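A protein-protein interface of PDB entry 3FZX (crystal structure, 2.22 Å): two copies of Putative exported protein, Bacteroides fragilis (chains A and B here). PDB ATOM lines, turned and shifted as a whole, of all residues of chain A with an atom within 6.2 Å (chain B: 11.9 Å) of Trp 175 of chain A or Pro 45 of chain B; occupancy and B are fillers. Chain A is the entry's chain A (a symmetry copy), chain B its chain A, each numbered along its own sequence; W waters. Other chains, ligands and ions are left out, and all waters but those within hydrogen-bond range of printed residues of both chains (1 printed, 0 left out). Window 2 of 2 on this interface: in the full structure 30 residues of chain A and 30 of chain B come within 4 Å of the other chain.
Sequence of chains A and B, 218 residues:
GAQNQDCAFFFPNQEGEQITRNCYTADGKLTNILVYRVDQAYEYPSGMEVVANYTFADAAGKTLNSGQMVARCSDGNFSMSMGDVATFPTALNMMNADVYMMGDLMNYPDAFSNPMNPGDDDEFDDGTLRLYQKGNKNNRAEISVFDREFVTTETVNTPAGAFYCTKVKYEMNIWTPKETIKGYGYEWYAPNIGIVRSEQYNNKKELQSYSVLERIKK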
ATOM      1  N   THR A  90      25.160 -29.022 -15.388  1.00  0.00           N
ATOM      2  CA  THR A  90      25.073 -27.645 -14.862  1.00  0.00           C
ATOM      3  C   THR A  90      23.718 -27.436 -14.228  1.00  0.00           C
ATOM      4  O   THR A  90      23.617 -26.876 -13.156  1.00  0.00           O
ATOM      5  CB  THR A  90      25.333 -26.573 -15.974  1.00  0.00           C
ATOM      6  OG1 THR A  90      26.639 -26.779 -16.513  1.00  0.00           O
ATOM      7  CG2 THR A  90      25.238 -25.143 -15.441  1.00  0.00           C
ATOM      8  N   ARG A 130      15.307 -21.620 -18.877  1.00  0.00           N
ATOM      9  CA  ARG A 130      15.969 -20.823 -17.847  1.00  0.00           C
ATOM     10  C   ARG A 130      15.607 -21.376 -16.471  1.00  0.00           C
ATOM     11  O   ARG A 130      14.441 -21.683 -16.217  1.00  0.00           O
ATOM     12  CB  ARG A 130      15.573 -19.348 -17.980  1.00  0.00           C
ATOM     13  CG  ARG A 130      16.238 -18.684 -19.234  1.00  0.00           C
ATOM     14  CD  ARG A 130      15.655 -17.362 -19.532  1.00  0.00           C
ATOM     15  NE  ARG A 130      16.416 -16.625 -20.537  1.00  0.00           N
ATOM     16  CZ  ARG A 130      16.101 -15.428 -21.015  1.00  0.00           C
ATOM     17  NH1 ARG A 130      14.994 -14.802 -20.624  1.00  0.00           N
ATOM     18  NH2 ARG A 130      16.899 -14.846 -21.905  1.00  0.00           N
ATOM     19  N   ARG A 140      21.340 -18.973 -10.986  1.00  0.00           N
ATOM     20  CA  ARG A 140      20.498 -19.153 -12.162  1.00  0.00           C
ATOM     21  C   ARG A 140      21.285 -19.680 -13.360  1.00  0.00           C
ATOM     22  O   ARG A 140      22.516 -19.643 -13.372  1.00  0.00           O
ATOM     23  CB  ARG A 140      19.825 -17.840 -12.529  1.00  0.00           C
ATOM     24  CG  ARG A 140      20.729 -16.734 -12.935  1.00  0.00           C
ATOM     25  CD  ARG A 140      19.927 -15.462 -13.075  1.00  0.00           C
ATOM     26  NE  ARG A 140      20.706 -14.391 -13.687  1.00  0.00           N
ATOM     27  CZ  ARG A 140      21.659 -13.685 -13.066  1.00  0.00           C
ATOM     28  NH1 ARG A 140      22.022 -13.933 -11.811  1.00  0.00           N
ATOM     29  NH2 ARG A 140      22.284 -12.745 -13.721  1.00  0.00           N
ATOM     30  N   ALA A 141      20.560 -20.125 -14.380  1.00  0.00           N
ATOM     31  CA  ALA A 141      21.176 -20.703 -15.560  1.00  0.00           C
ATOM     32  C   ALA A 141      20.250 -20.558 -16.756  1.00  0.00           C
ATOM     33  O   ALA A 141      19.041 -20.467 -16.588  1.00  0.00           O
ATOM     34  CB  ALA A 141      21.466 -22.192 -15.297  1.00  0.00           C
ATOM     35  N   GLU A 142      20.831 -20.549 -17.950  1.00  0.00           N
ATOM     36  CA  GLU A 142      20.091 -20.602 -19.209  1.00  0.00           C
ATOM     37  C   GLU A 142      20.654 -21.705 -20.108  1.00  0.00           C
ATOM     38  O   GLU A 142      21.883 -21.764 -20.330  1.00  0.00           O
ATOM     39  CB  GLU A 142      20.183 -19.285 -19.939  1.00  0.00           C
ATOM     40  CG  GLU A 142      19.454 -19.267 -21.292  1.00  0.00           C
ATOM     41  CD  GLU A 142      19.577 -17.927 -21.998  1.00  0.00           C
ATOM     42  OE1 GLU A 142      18.795 -17.006 -21.720  1.00  0.00           O
ATOM     43  OE2 GLU A 142      20.453 -17.792 -22.862  1.00  0.00           O
ATOM     44  N   ILE A 143      19.774 -22.575 -20.614  1.00  0.00           N
ATOM     45  CA  ILE A 143      20.178 -23.622 -21.579  1.00  0.00           C
ATOM     46  C   ILE A 143      19.456 -23.397 -22.909  1.00  0.00           C
ATOM     47  O   ILE A 143      18.227 -23.539 -22.997  1.00  0.00           O
ATOM     48  CB  ILE A 143      19.895 -25.060 -21.100  1.00  0.00           C
ATOM     49  CG1 ILE A 143      20.547 -25.344 -19.733  1.00  0.00           C
ATOM     50  CG2 ILE A 143      20.477 -26.083 -22.127  1.00  0.00           C
ATOM     51  CD1 ILE A 143      20.034 -26.620 -19.051  1.00  0.00           C
ATOM     52  N   ASN A 173      24.041 -23.976 -25.838  1.00  0.00           N
ATOM     53  CA  ASN A 173      24.798 -22.985 -25.090  1.00  0.00           C
ATOM     54  C   ASN A 173      24.243 -23.007 -23.676  1.00  0.00           C
ATOM     55  O   ASN A 173      23.022 -22.980 -23.478  1.00  0.00           O
ATOM     56  CB  ASN A 173      24.648 -21.593 -25.706  1.00  0.00           C
ATOM     57  CG  ASN A 173      25.334 -21.476 -27.060  1.00  0.00           C
ATOM     58  OD1 ASN A 173      26.062 -22.376 -27.485  1.00  0.00           O
ATOM     59  ND2 ASN A 173      25.107 -20.363 -27.740  1.00  0.00           N
ATOM     60  N   ILE A 174      25.139 -23.110 -22.697  1.00  0.00           N
ATOM     61  CA  ILE A 174      24.760 -23.133 -21.287  1.00  0.00           C
ATOM     62  C   ILE A 174      25.477 -21.981 -20.592  1.00  0.00           C
ATOM     63  O   ILE A 174      26.702 -21.925 -20.596  1.00  0.00           O
ATOM     64  CB  ILE A 174      25.193 -24.421 -20.624  1.00  0.00           C
ATOM     65  CG1 ILE A 174      24.596 -25.620 -21.361  1.00  0.00           C
ATOM     66  CG2 ILE A 174      24.847 -24.374 -19.124  1.00  0.00           C
ATOM     67  CD1 ILE A 174      25.400 -26.895 -21.193  1.00  0.00           C
ATOM     68  N   TRP A 175      24.719 -21.057 -20.029  1.00  0.00           N
ATOM     69  CA  TRP A 175      25.272 -19.918 -19.346  1.00  0.00           C
ATOM     70  C   TRP A 175      24.822 -19.909 -17.902  1.00  0.00           C
ATOM     71  O   TRP A 175      23.671 -20.189 -17.617  1.00  0.00           O
ATOM     72  CB  TRP A 175      24.785 -18.663 -20.009  1.00  0.00           C
ATOM     73  CG  TRP A 175      25.291 -17.428 -19.322  1.00  0.00           C
ATOM     74  CD1 TRP A 175      26.446 -16.789 -19.582  1.00  0.00           C
ATOM     75  CD2 TRP A 175      24.663 -16.706 -18.245  1.00  0.00           C
ATOM     76  NE1 TRP A 175      26.592 -15.718 -18.757  1.00  0.00           N
ATOM     77  CE2 TRP A 175      25.517 -15.639 -17.915  1.00  0.00           C
ATOM     78  CE3 TRP A 175      23.473 -16.870 -17.523  1.00  0.00           C
ATOM     79  CZ2 TRP A 175      25.214 -14.703 -16.899  1.00  0.00           C
ATOM     80  CZ3 TRP A 175      23.171 -15.953 -16.505  1.00  0.00           C
ATOM     81  CH2 TRP A 175      24.045 -14.888 -16.198  1.00  0.00           C
ATOM     82  N   THR A 176      25.753 -19.640 -16.997  1.00  0.00           N
ATOM     83  CA  THR A 176      25.462 -19.275 -15.605  1.00  0.00           C
ATOM     84  C   THR A 176      26.307 -18.030 -15.390  1.00  0.00           C
ATOM     85  O   THR A 176      27.151 -17.714 -16.230  1.00  0.00           O
ATOM     86  CB  THR A 176      25.916 -20.317 -14.560  1.00  0.00           C
ATOM     87  OG1 THR A 176      27.356 -20.327 -14.484  1.00  0.00           O
ATOM     88  CG2 THR A 176      25.391 -21.673 -14.887  1.00  0.00           C
ATOM     89  N   PRO A 177      26.066 -17.298 -14.283  1.00  0.00           N
ATOM     90  CA  PRO A 177      26.925 -16.143 -13.989  1.00  0.00           C
ATOM     91  C   PRO A 177      28.407 -16.507 -13.823  1.00  0.00           C
ATOM     92  O   PRO A 177      29.235 -15.642 -13.991  1.00  0.00           O
ATOM     93  CB  PRO A 177      26.362 -15.613 -12.667  1.00  0.00           C
ATOM     94  CG  PRO A 177      24.937 -16.090 -12.664  1.00  0.00           C
ATOM     95  CD  PRO A 177      24.959 -17.415 -13.315  1.00  0.00           C
ATOM     96  N   LYS A 178      28.719 -17.763 -13.498  1.00  0.00           N
ATOM     97  CA  LYS A 178      30.104 -18.212 -13.355  1.00  0.00           C
ATOM     98  C   LYS A 178      30.758 -18.726 -14.641  1.00  0.00           C
ATOM     99  O   LYS A 178      31.979 -18.695 -14.730  1.00  0.00           O
ATOM    100  CB  LYS A 178      30.218 -19.267 -12.242  1.00  0.00           C
ATOM    101  CG  LYS A 178      30.021 -18.625 -10.855  1.00  0.00           C
ATOM    102  CD  LYS A 178      30.023 -19.607  -9.681  1.00  0.00           C
ATOM    103  CE  LYS A 178      30.098 -18.827  -8.363  1.00  0.00           C
ATOM    104  NZ  LYS A 178      30.071 -19.668  -7.126  1.00  0.00           N
ATOM    105  N   GLU A 179      29.983 -19.185 -15.634  1.00  0.00           N
ATOM    106  CA  GLU A 179      30.574 -19.705 -16.892  1.00  0.00           C
ATOM    107  C   GLU A 179      29.624 -19.966 -18.064  1.00  0.00           C
ATOM    108  O   GLU A 179      28.432 -20.167 -17.872  1.00  0.00           O
ATOM    109  CB  GLU A 179      31.305 -21.016 -16.624  1.00  0.00           C
ATOM    110  CG  GLU A 179      30.483 -22.051 -15.881  1.00  0.00           C
ATOM    111  CD  GLU A 179      31.168 -23.403 -15.835  1.00  0.00           C
ATOM    112  OE1 GLU A 179      32.334 -23.506 -16.278  1.00  0.00           O
ATOM    113  OE2 GLU A 179      30.535 -24.373 -15.367  1.00  0.00           O
ATOM    114  N   THR A 180      30.200 -19.958 -19.268  1.00  0.00           N
ATOM    115  CA  THR A 180      29.538 -20.365 -20.494  1.00  0.00           C
ATOM    116  C   THR A 180      30.162 -21.655 -20.958  1.00  0.00           C
ATOM    117  O   THR A 180      31.370 -21.737 -21.047  1.00  0.00           O
ATOM    118  CB  THR A 180      29.732 -19.367 -21.628  1.00  0.00           C
ATOM    119  OG1 THR A 180      29.133 -18.128 -21.266  1.00  0.00           O
ATOM    120  CG2 THR A 180      29.066 -19.871 -22.922  1.00  0.00           C
ATOM    121  N   ILE A 181      29.329 -22.650 -21.246  1.00  0.00           N
ATOM    122  CA  ILE A 181      29.756 -23.911 -21.826  1.00  0.00           C
ATOM    123  C   ILE A 181      29.075 -23.971 -23.197  1.00  0.00           C
ATOM    124  O   ILE A 181      27.899 -23.664 -23.302  1.00  0.00           O
ATOM    125  CB  ILE A 181      29.277 -25.113 -20.992  1.00  0.00           C
ATOM    126  CG1 ILE A 181      29.796 -25.044 -19.558  1.00  0.00           C
ATOM    127  CG2 ILE A 181      29.734 -26.429 -21.615  1.00  0.00           C
ATOM    128  CD1 ILE A 181      29.179 -26.143 -18.701  1.00  0.00           C
ATOM    129  N   CYS B   7      15.437  -3.803 -28.516  1.00  0.00           N
ATOM    130  CA  CYS B   7      14.769  -4.998 -27.915  1.00  0.00           C
ATOM    131  C   CYS B   7      13.772  -4.529 -26.850  1.00  0.00           C
ATOM    132  O   CYS B   7      14.105  -4.437 -25.669  1.00  0.00           O
ATOM    133  CB  CYS B   7      15.810  -5.950 -27.311  1.00  0.00           C
ATOM    134  N   PHE B   9      10.538  -4.737 -24.333  1.00  0.00           N
ATOM    135  CA  PHE B   9      10.029  -5.791 -23.457  1.00  0.00           C
ATOM    136  C   PHE B   9       8.560  -5.451 -23.187  1.00  0.00           C
ATOM    137  O   PHE B   9       8.264  -4.505 -22.474  1.00  0.00           O
ATOM    138  CB  PHE B   9      10.885  -5.828 -22.175  1.00  0.00           C
ATOM    139  CG  PHE B   9      10.703  -7.060 -21.341  1.00  0.00           C
ATOM    140  CD1 PHE B   9       9.739  -7.102 -20.348  1.00  0.00           C
ATOM    141  CD2 PHE B   9      11.527  -8.159 -21.515  1.00  0.00           C
ATOM    142  CE1 PHE B   9       9.562  -8.236 -19.566  1.00  0.00           C
ATOM    143  CE2 PHE B   9      11.369  -9.315 -20.742  1.00  0.00           C
ATOM    144  CZ  PHE B   9      10.396  -9.352 -19.746  1.00  0.00           C
ATOM    145  N   ALA B  41      12.693 -10.164 -11.524  1.00  0.00           N
ATOM    146  CA  ALA B  41      13.272  -9.915 -12.843  1.00  0.00           C
ATOM    147  C   ALA B  41      14.686 -10.457 -12.790  1.00  0.00           C
ATOM    148  O   ALA B  41      15.413 -10.148 -11.864  1.00  0.00           O
ATOM    149  CB  ALA B  41      13.273  -8.473 -13.161  1.00  0.00           C
ATOM    150  N   TYR B  42      15.058 -11.289 -13.760  1.00  0.00           N
ATOM    151  CA  TYR B  42      16.386 -11.887 -13.845  1.00  0.00           C
ATOM    152  C   TYR B  42      17.060 -11.468 -15.144  1.00  0.00           C
ATOM    153  O   TYR B  42      16.427 -11.446 -16.209  1.00  0.00           O
ATOM    154  CB  TYR B  42      16.261 -13.410 -13.857  1.00  0.00           C
ATOM    155  CG  TYR B  42      15.561 -13.993 -12.650  1.00  0.00           C
ATOM    156  CD1 TYR B  42      16.269 -14.300 -11.492  1.00  0.00           C
ATOM    157  CD2 TYR B  42      14.192 -14.236 -12.662  1.00  0.00           C
ATOM    158  CE1 TYR B  42      15.626 -14.843 -10.378  1.00  0.00           C
ATOM    159  CE2 TYR B  42      13.539 -14.775 -11.549  1.00  0.00           C
ATOM    160  CZ  TYR B  42      14.264 -15.080 -10.412  1.00  0.00           C
ATOM    161  OH  TYR B  42      13.634 -15.605  -9.304  1.00  0.00           O
ATOM    162  N   GLU B  43      18.360 -11.203 -15.076  1.00  0.00           N
ATOM    163  CA  GLU B  43      19.113 -10.791 -16.244  1.00  0.00           C
ATOM    164  C   GLU B  43      19.930 -11.935 -16.773  1.00  0.00           C
ATOM    165  O   GLU B  43      20.591 -12.636 -16.017  1.00  0.00           O
ATOM    166  CB  GLU B  43      20.030  -9.625 -15.882  1.00  0.00           C
ATOM    167  CG  GLU B  43      19.242  -8.315 -15.734  1.00  0.00           C
ATOM    168  CD  GLU B  43      19.836  -7.349 -14.705  1.00  0.00           C
ATOM    169  OE1 GLU B  43      21.000  -7.530 -14.272  1.00  0.00           O
ATOM    170  OE2 GLU B  43      19.121  -6.390 -14.327  1.00  0.00           O
ATOM    171  N   TYR B  44      19.854 -12.126 -18.083  1.00  0.00           N
ATOM    172  CA  TYR B  44      20.627 -13.114 -18.790  1.00  0.00           C
ATOM    173  C   TYR B  44      21.348 -12.376 -19.915  1.00  0.00           C
ATOM    174  O   TYR B  44      20.874 -11.347 -20.374  1.00  0.00           O
ATOM    175  CB  TYR B  44      19.709 -14.203 -19.349  1.00  0.00           C
ATOM    176  CG  TYR B  44      19.146 -15.126 -18.296  1.00  0.00           C
ATOM    177  CD1 TYR B  44      19.838 -16.278 -17.930  1.00  0.00           C
ATOM    178  CD2 TYR B  44      17.942 -14.843 -17.640  1.00  0.00           C
ATOM    179  CE1 TYR B  44      19.349 -17.130 -16.956  1.00  0.00           C
ATOM    180  CE2 TYR B  44      17.442 -15.709 -16.647  1.00  0.00           C
ATOM    181  CZ  TYR B  44      18.150 -16.845 -16.333  1.00  0.00           C
ATOM    182  OH  TYR B  44      17.695 -17.708 -15.382  1.00  0.00           O
ATOM    183  N   PRO B  45      22.502 -12.890 -20.367  1.00  0.00           N
ATOM    184  CA  PRO B  45      23.190 -12.200 -21.462  1.00  0.00           C
ATOM    185  C   PRO B  45      22.251 -11.950 -22.643  1.00  0.00           C
ATOM    186  O   PRO B  45      22.186 -10.848 -23.153  1.00  0.00           O
ATOM    187  CB  PRO B  45      24.307 -13.178 -21.858  1.00  0.00           C
ATOM    188  CG  PRO B  45      24.417 -14.151 -20.723  1.00  0.00           C
ATOM    189  CD  PRO B  45      23.055 -14.234 -20.131  1.00  0.00           C
ATOM    190  N   SER B  46      21.462 -12.949 -23.006  1.00  0.00           N
ATOM    191  CA  SER B  46      20.553 -12.844 -24.150  1.00  0.00           C
ATOM    192  C   SER B  46      19.269 -12.032 -23.930  1.00  0.00           C
ATOM    193  O   SER B  46      18.403 -12.036 -24.817  1.00  0.00           O
ATOM    194  CB  SER B  46      20.146 -14.257 -24.569  1.00  0.00           C
ATOM    195  OG  SER B  46      19.424 -14.863 -23.516  1.00  0.00           O
ATOM    196  N   GLY B  47      19.124 -11.353 -22.788  1.00  0.00           N
ATOM    197  CA  GLY B  47      17.858 -10.697 -22.448  1.00  0.00           C
ATOM    198  C   GLY B  47      17.330 -11.050 -21.059  1.00  0.00           C
ATOM    199  O   GLY B  47      17.946 -11.780 -20.308  1.00  0.00           O
ATOM    200  N   MET B  48      16.157 -10.551 -20.742  1.00  0.00           N
ATOM    201  CA  MET B  48      15.592 -10.619 -19.398  1.00  0.00           C
ATOM    202  C   MET B  48      14.486 -11.674 -19.233  1.00  0.00           C
ATOM    203  O   MET B  48      13.792 -12.017 -20.190  1.00  0.00           O
ATOM    204  CB  MET B  48      15.018  -9.229 -19.115  1.00  0.00           C
ATOM    205  CG  MET B  48      14.214  -9.031 -17.866  1.00  0.00           C
ATOM    206  SD  MET B  48      14.274  -7.061 -17.450  1.00  0.00           S
ATOM    207  CE  MET B  48      13.461  -6.400 -19.122  1.00  0.00           C
ATOM    208  N   GLU B  49      14.334 -12.163 -18.003  1.00  0.00           N
ATOM    209  CA  GLU B  49      13.266 -13.070 -17.619  1.00  0.00           C
ATOM    210  C   GLU B  49      12.478 -12.427 -16.478  1.00  0.00           C
ATOM    211  O   GLU B  49      13.073 -12.033 -15.468  1.00  0.00           O
ATOM    212  CB  GLU B  49      13.833 -14.385 -17.111  1.00  0.00           C
ATOM    213  CG  GLU B  49      12.774 -15.462 -16.878  1.00  0.00           C
ATOM    214  CD  GLU B  49      12.600 -16.378 -18.071  1.00  0.00           C
ATOM    215  OE1 GLU B  49      12.914 -15.966 -19.216  1.00  0.00           O
ATOM    216  OE2 GLU B  49      12.160 -17.538 -17.857  1.00  0.00           O
ATOM    217  N   ARG B  72       9.537 -12.811 -21.297  1.00  0.00           N
ATOM    218  CA  ARG B  72      10.950 -12.897 -21.580  1.00  0.00           C
ATOM    219  C   ARG B  72      11.425 -12.350 -22.917  1.00  0.00           C
ATOM    220  O   ARG B  72      10.702 -12.352 -23.904  1.00  0.00           O
ATOM    221  CB  ARG B  72      11.466 -14.345 -21.467  1.00  0.00           C
ATOM    222  CG  ARG B  72      10.970 -15.292 -22.524  1.00  0.00           C
ATOM    223  CD  ARG B  72      11.782 -16.607 -22.667  1.00  0.00           C
ATOM    224  NE  ARG B  72      11.933 -17.362 -21.427  1.00  0.00           N
ATOM    225  CZ  ARG B  72      12.230 -18.662 -21.348  1.00  0.00           C
ATOM    226  NH1 ARG B  72      12.328 -19.423 -22.434  1.00  0.00           N
ATOM    227  NH2 ARG B  72      12.384 -19.226 -20.155  1.00  0.00           N
ATOM    228  N   CYS B  73      12.692 -11.952 -22.895  1.00  0.00           N
ATOM    229  CA  CYS B  73      13.436 -11.505 -24.044  1.00  0.00           C
ATOM    230  C   CYS B  73      14.562 -12.501 -24.211  1.00  0.00           C
ATOM    231  O   CYS B  73      15.303 -12.760 -23.278  1.00  0.00           O
ATOM    232  CB  CYS B  73      14.034 -10.120 -23.762  1.00  0.00           C
ATOM    233  SG  CYS B  73      13.898  -9.058 -25.125  1.00  0.00           S
ATOM    234  N   SER B  74      14.653 -13.090 -25.384  1.00  0.00           N
ATOM    235  CA  SER B  74      15.763 -13.943 -25.728  1.00  0.00           C
ATOM    236  C   SER B  74      16.273 -13.565 -27.125  1.00  0.00           C
ATOM    237  O   SER B  74      15.525 -13.586 -28.104  1.00  0.00           O
ATOM    238  CB  SER B  74      15.369 -15.391 -25.684  1.00  0.00           C
ATOM    239  OG  SER B  74      16.490 -16.128 -26.117  1.00  0.00           O
ATOM    240  N   ASP B  75      17.555 -13.227 -27.194  1.00  0.00           N
ATOM    241  CA  ASP B  75      18.162 -12.627 -28.376  1.00  0.00           C
ATOM    242  C   ASP B  75      17.359 -11.365 -28.656  1.00  0.00           C
ATOM    243  O   ASP B  75      17.131 -10.569 -27.722  1.00  0.00           O
ATOM    244  CB  ASP B  75      18.268 -13.624 -29.542  1.00  0.00           C
ATOM    245  CG  ASP B  75      19.376 -14.670 -29.321  1.00  0.00           C
ATOM    246  OD1 ASP B  75      20.298 -14.432 -28.496  1.00  0.00           O
ATOM    247  OD2 ASP B  75      19.328 -15.731 -29.990  1.00  0.00           O
ATOM    248  N   GLY B  76      16.885 -11.146 -29.867  1.00  0.00           N
ATOM    249  CA  GLY B  76      16.102  -9.934 -30.086  1.00  0.00           C
ATOM    250  C   GLY B  76      14.630 -10.063 -29.745  1.00  0.00           C
ATOM    251  O   GLY B  76      13.921  -9.055 -29.782  1.00  0.00           O
ATOM    252  N   ASN B  77      14.187 -11.262 -29.343  1.00  0.00           N
ATOM    253  CA  ASN B  77      12.766 -11.631 -29.365  1.00  0.00           C
ATOM    254  C   ASN B  77      12.037 -11.762 -28.045  1.00  0.00           C
ATOM    255  O   ASN B  77      12.436 -12.519 -27.144  1.00  0.00           O
ATOM    256  CB  ASN B  77      12.628 -12.914 -30.176  1.00  0.00           C
ATOM    257  CG  ASN B  77      13.473 -12.858 -31.459  1.00  0.00           C
ATOM    258  OD1 ASN B  77      13.628 -11.789 -32.066  1.00  0.00           O
ATOM    259  ND2 ASN B  77      14.067 -13.982 -31.833  1.00  0.00           N
HETATM  260  O   HOH W   1      19.643 -11.052 -12.567  1.00  0.00           O
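The guanidinium group (NH2) of Arg 140 of chain A is in hydrogen-bond range of the backbone carbonyl oxygen (O) of Glu 43 of chain B (2.9 Å). OH of Tyr 44 of chain B sits at hydrogen-bond distance from O of Ala 141 of chain A. The side-chain hydroxyl (OG) of Ser 46 of chain B sits at hydrogen-bond distance from the guanidinium group (NH2) of Arg 130 of chain A (3.0 Å). OE1 of Glu 142 of chain A is in hydrogen-bond range of OG of Ser 46 of chain B (2.9 Å). The guanidinium group (NH1) of Arg 130 of chain A lies within hydrogen-bond range of the backbone carbonyl oxygen (O) of Met 48 of chain B, at 3.1 Å. OE1 of Glu 49 of chain B is in salt-bridge range of NH1 of Arg 130 of chain A (2.8 Å). The backbone carbonyl oxygen of Cys 73 of chain B sits at hydrogen-bond distance from the guanidinium group of Arg 130 of chain A.
The backbone carbonyl oxygen of Glu 49 of chain B sits at hydrogen-bond distance from the backbone NH of Tyr 42 of chain B (2.7 Å). The backbone NH of Asp 75 of chain B is in hydrogen-bond range of the backbone carbonyl oxygen of Ser 46 of chain B, at 2.8 Å. The backbone carbonyl oxygen (O) of Met 48 of chain B sits at hydrogen-bond distance from the backbone NH (N) of Cys 73 of chain B, 2.9 Å away. The guanidinium group (NE) of Arg 72 of chain B is in salt-bridge range of the side-chain carboxylate (OE1) of Glu 49 of chain B, at 2.8 Å. The guanidinium group of Arg 130 of chain A is in salt-bridge range of the side-chain carboxylate of Glu 142 of chain A. O of Trp 175 of chain A is in hydrogen-bond range of N of Glu 142 of chain A, 2.9 Å away.
Among the printed residues, pairs that only touch across the chains: Arg 130 of chain A with Tyr 44 of chain B (3.7 Å), Arg 130 of chain A with Gly 47 of chain B (3.6 Å), Arg 130 of chain A with Arg 72 of chain B (3.7 Å), Arg 140 of chain A with Tyr 44 of chain B (3.6 Å), Glu 142 of chain A with Tyr 44 of chain B (3.6 Å), Trp 175 of chain A with Tyr 44 of chain B (3.6 Å) and Trp 175 of chain A with Pro 45 of chain B (3.3 Å).
Of the printed residues of chain B, Arg 130 of chain A touches Tyr 44 (3.7 Å), Ser 46 (3.0 Å), Gly 47 (3.6 Å), Met 48 (3.1 Å), Glu 49 (2.8 Å), Arg 72 (3.7 Å) and Cys 73 (3.0 Å). Of the printed residues of chain B, Arg 140 of chain A touches Glu 43 and Tyr 44. Of the printed residues of chain B, Ala 141 of chain A touches Tyr 44. No residue of chain B comes within 4 Å of Ile 174 of chain A. Trp 175 of chain A touches just these residues of chain B: Tyr 44 (3.6 Å) and Pro 45 (3.3 Å). No residue of chain B comes within 4 Å of Thr 180 of chain A. Pro 45 of chain B touches one residue of chain A. Of the printed residues of chain A, Ser 46 of chain B touches Arg 130 (3.0 Å) and Glu 142 (2.9 Å). Of the printed residues of chain A, Arg 72 of chain B touches Arg 130. Of the printed residues of chain A, Cys 73 of chain B touches Arg 130 (3.0 Å). Gly 76 of chain B touches none of the printed residues of chain A. The nearest residue of chain B that does not touch Trp 175 of chain A is Glu 43 of chain B (4.1 Å). The nearest residue of chain A that does not touch Pro 45 of chain B is Glu 142 of chain A (5.2 Å).
Hydrophobic or aromatic side chains of chain A that line the printed part of chain B: Trp 175.
No position is printed for both chains. Of the 14 pairs that touch across the chains among the printed residues, none has its exchanged pair printed and touching as well.
Water W1 lies within hydrogen-bond range of the backbone NH (N) of Glu 43 of chain B (2.8 Å) and the guanidinium group (NH2) of Arg 140 of chain A (3.3 Å).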
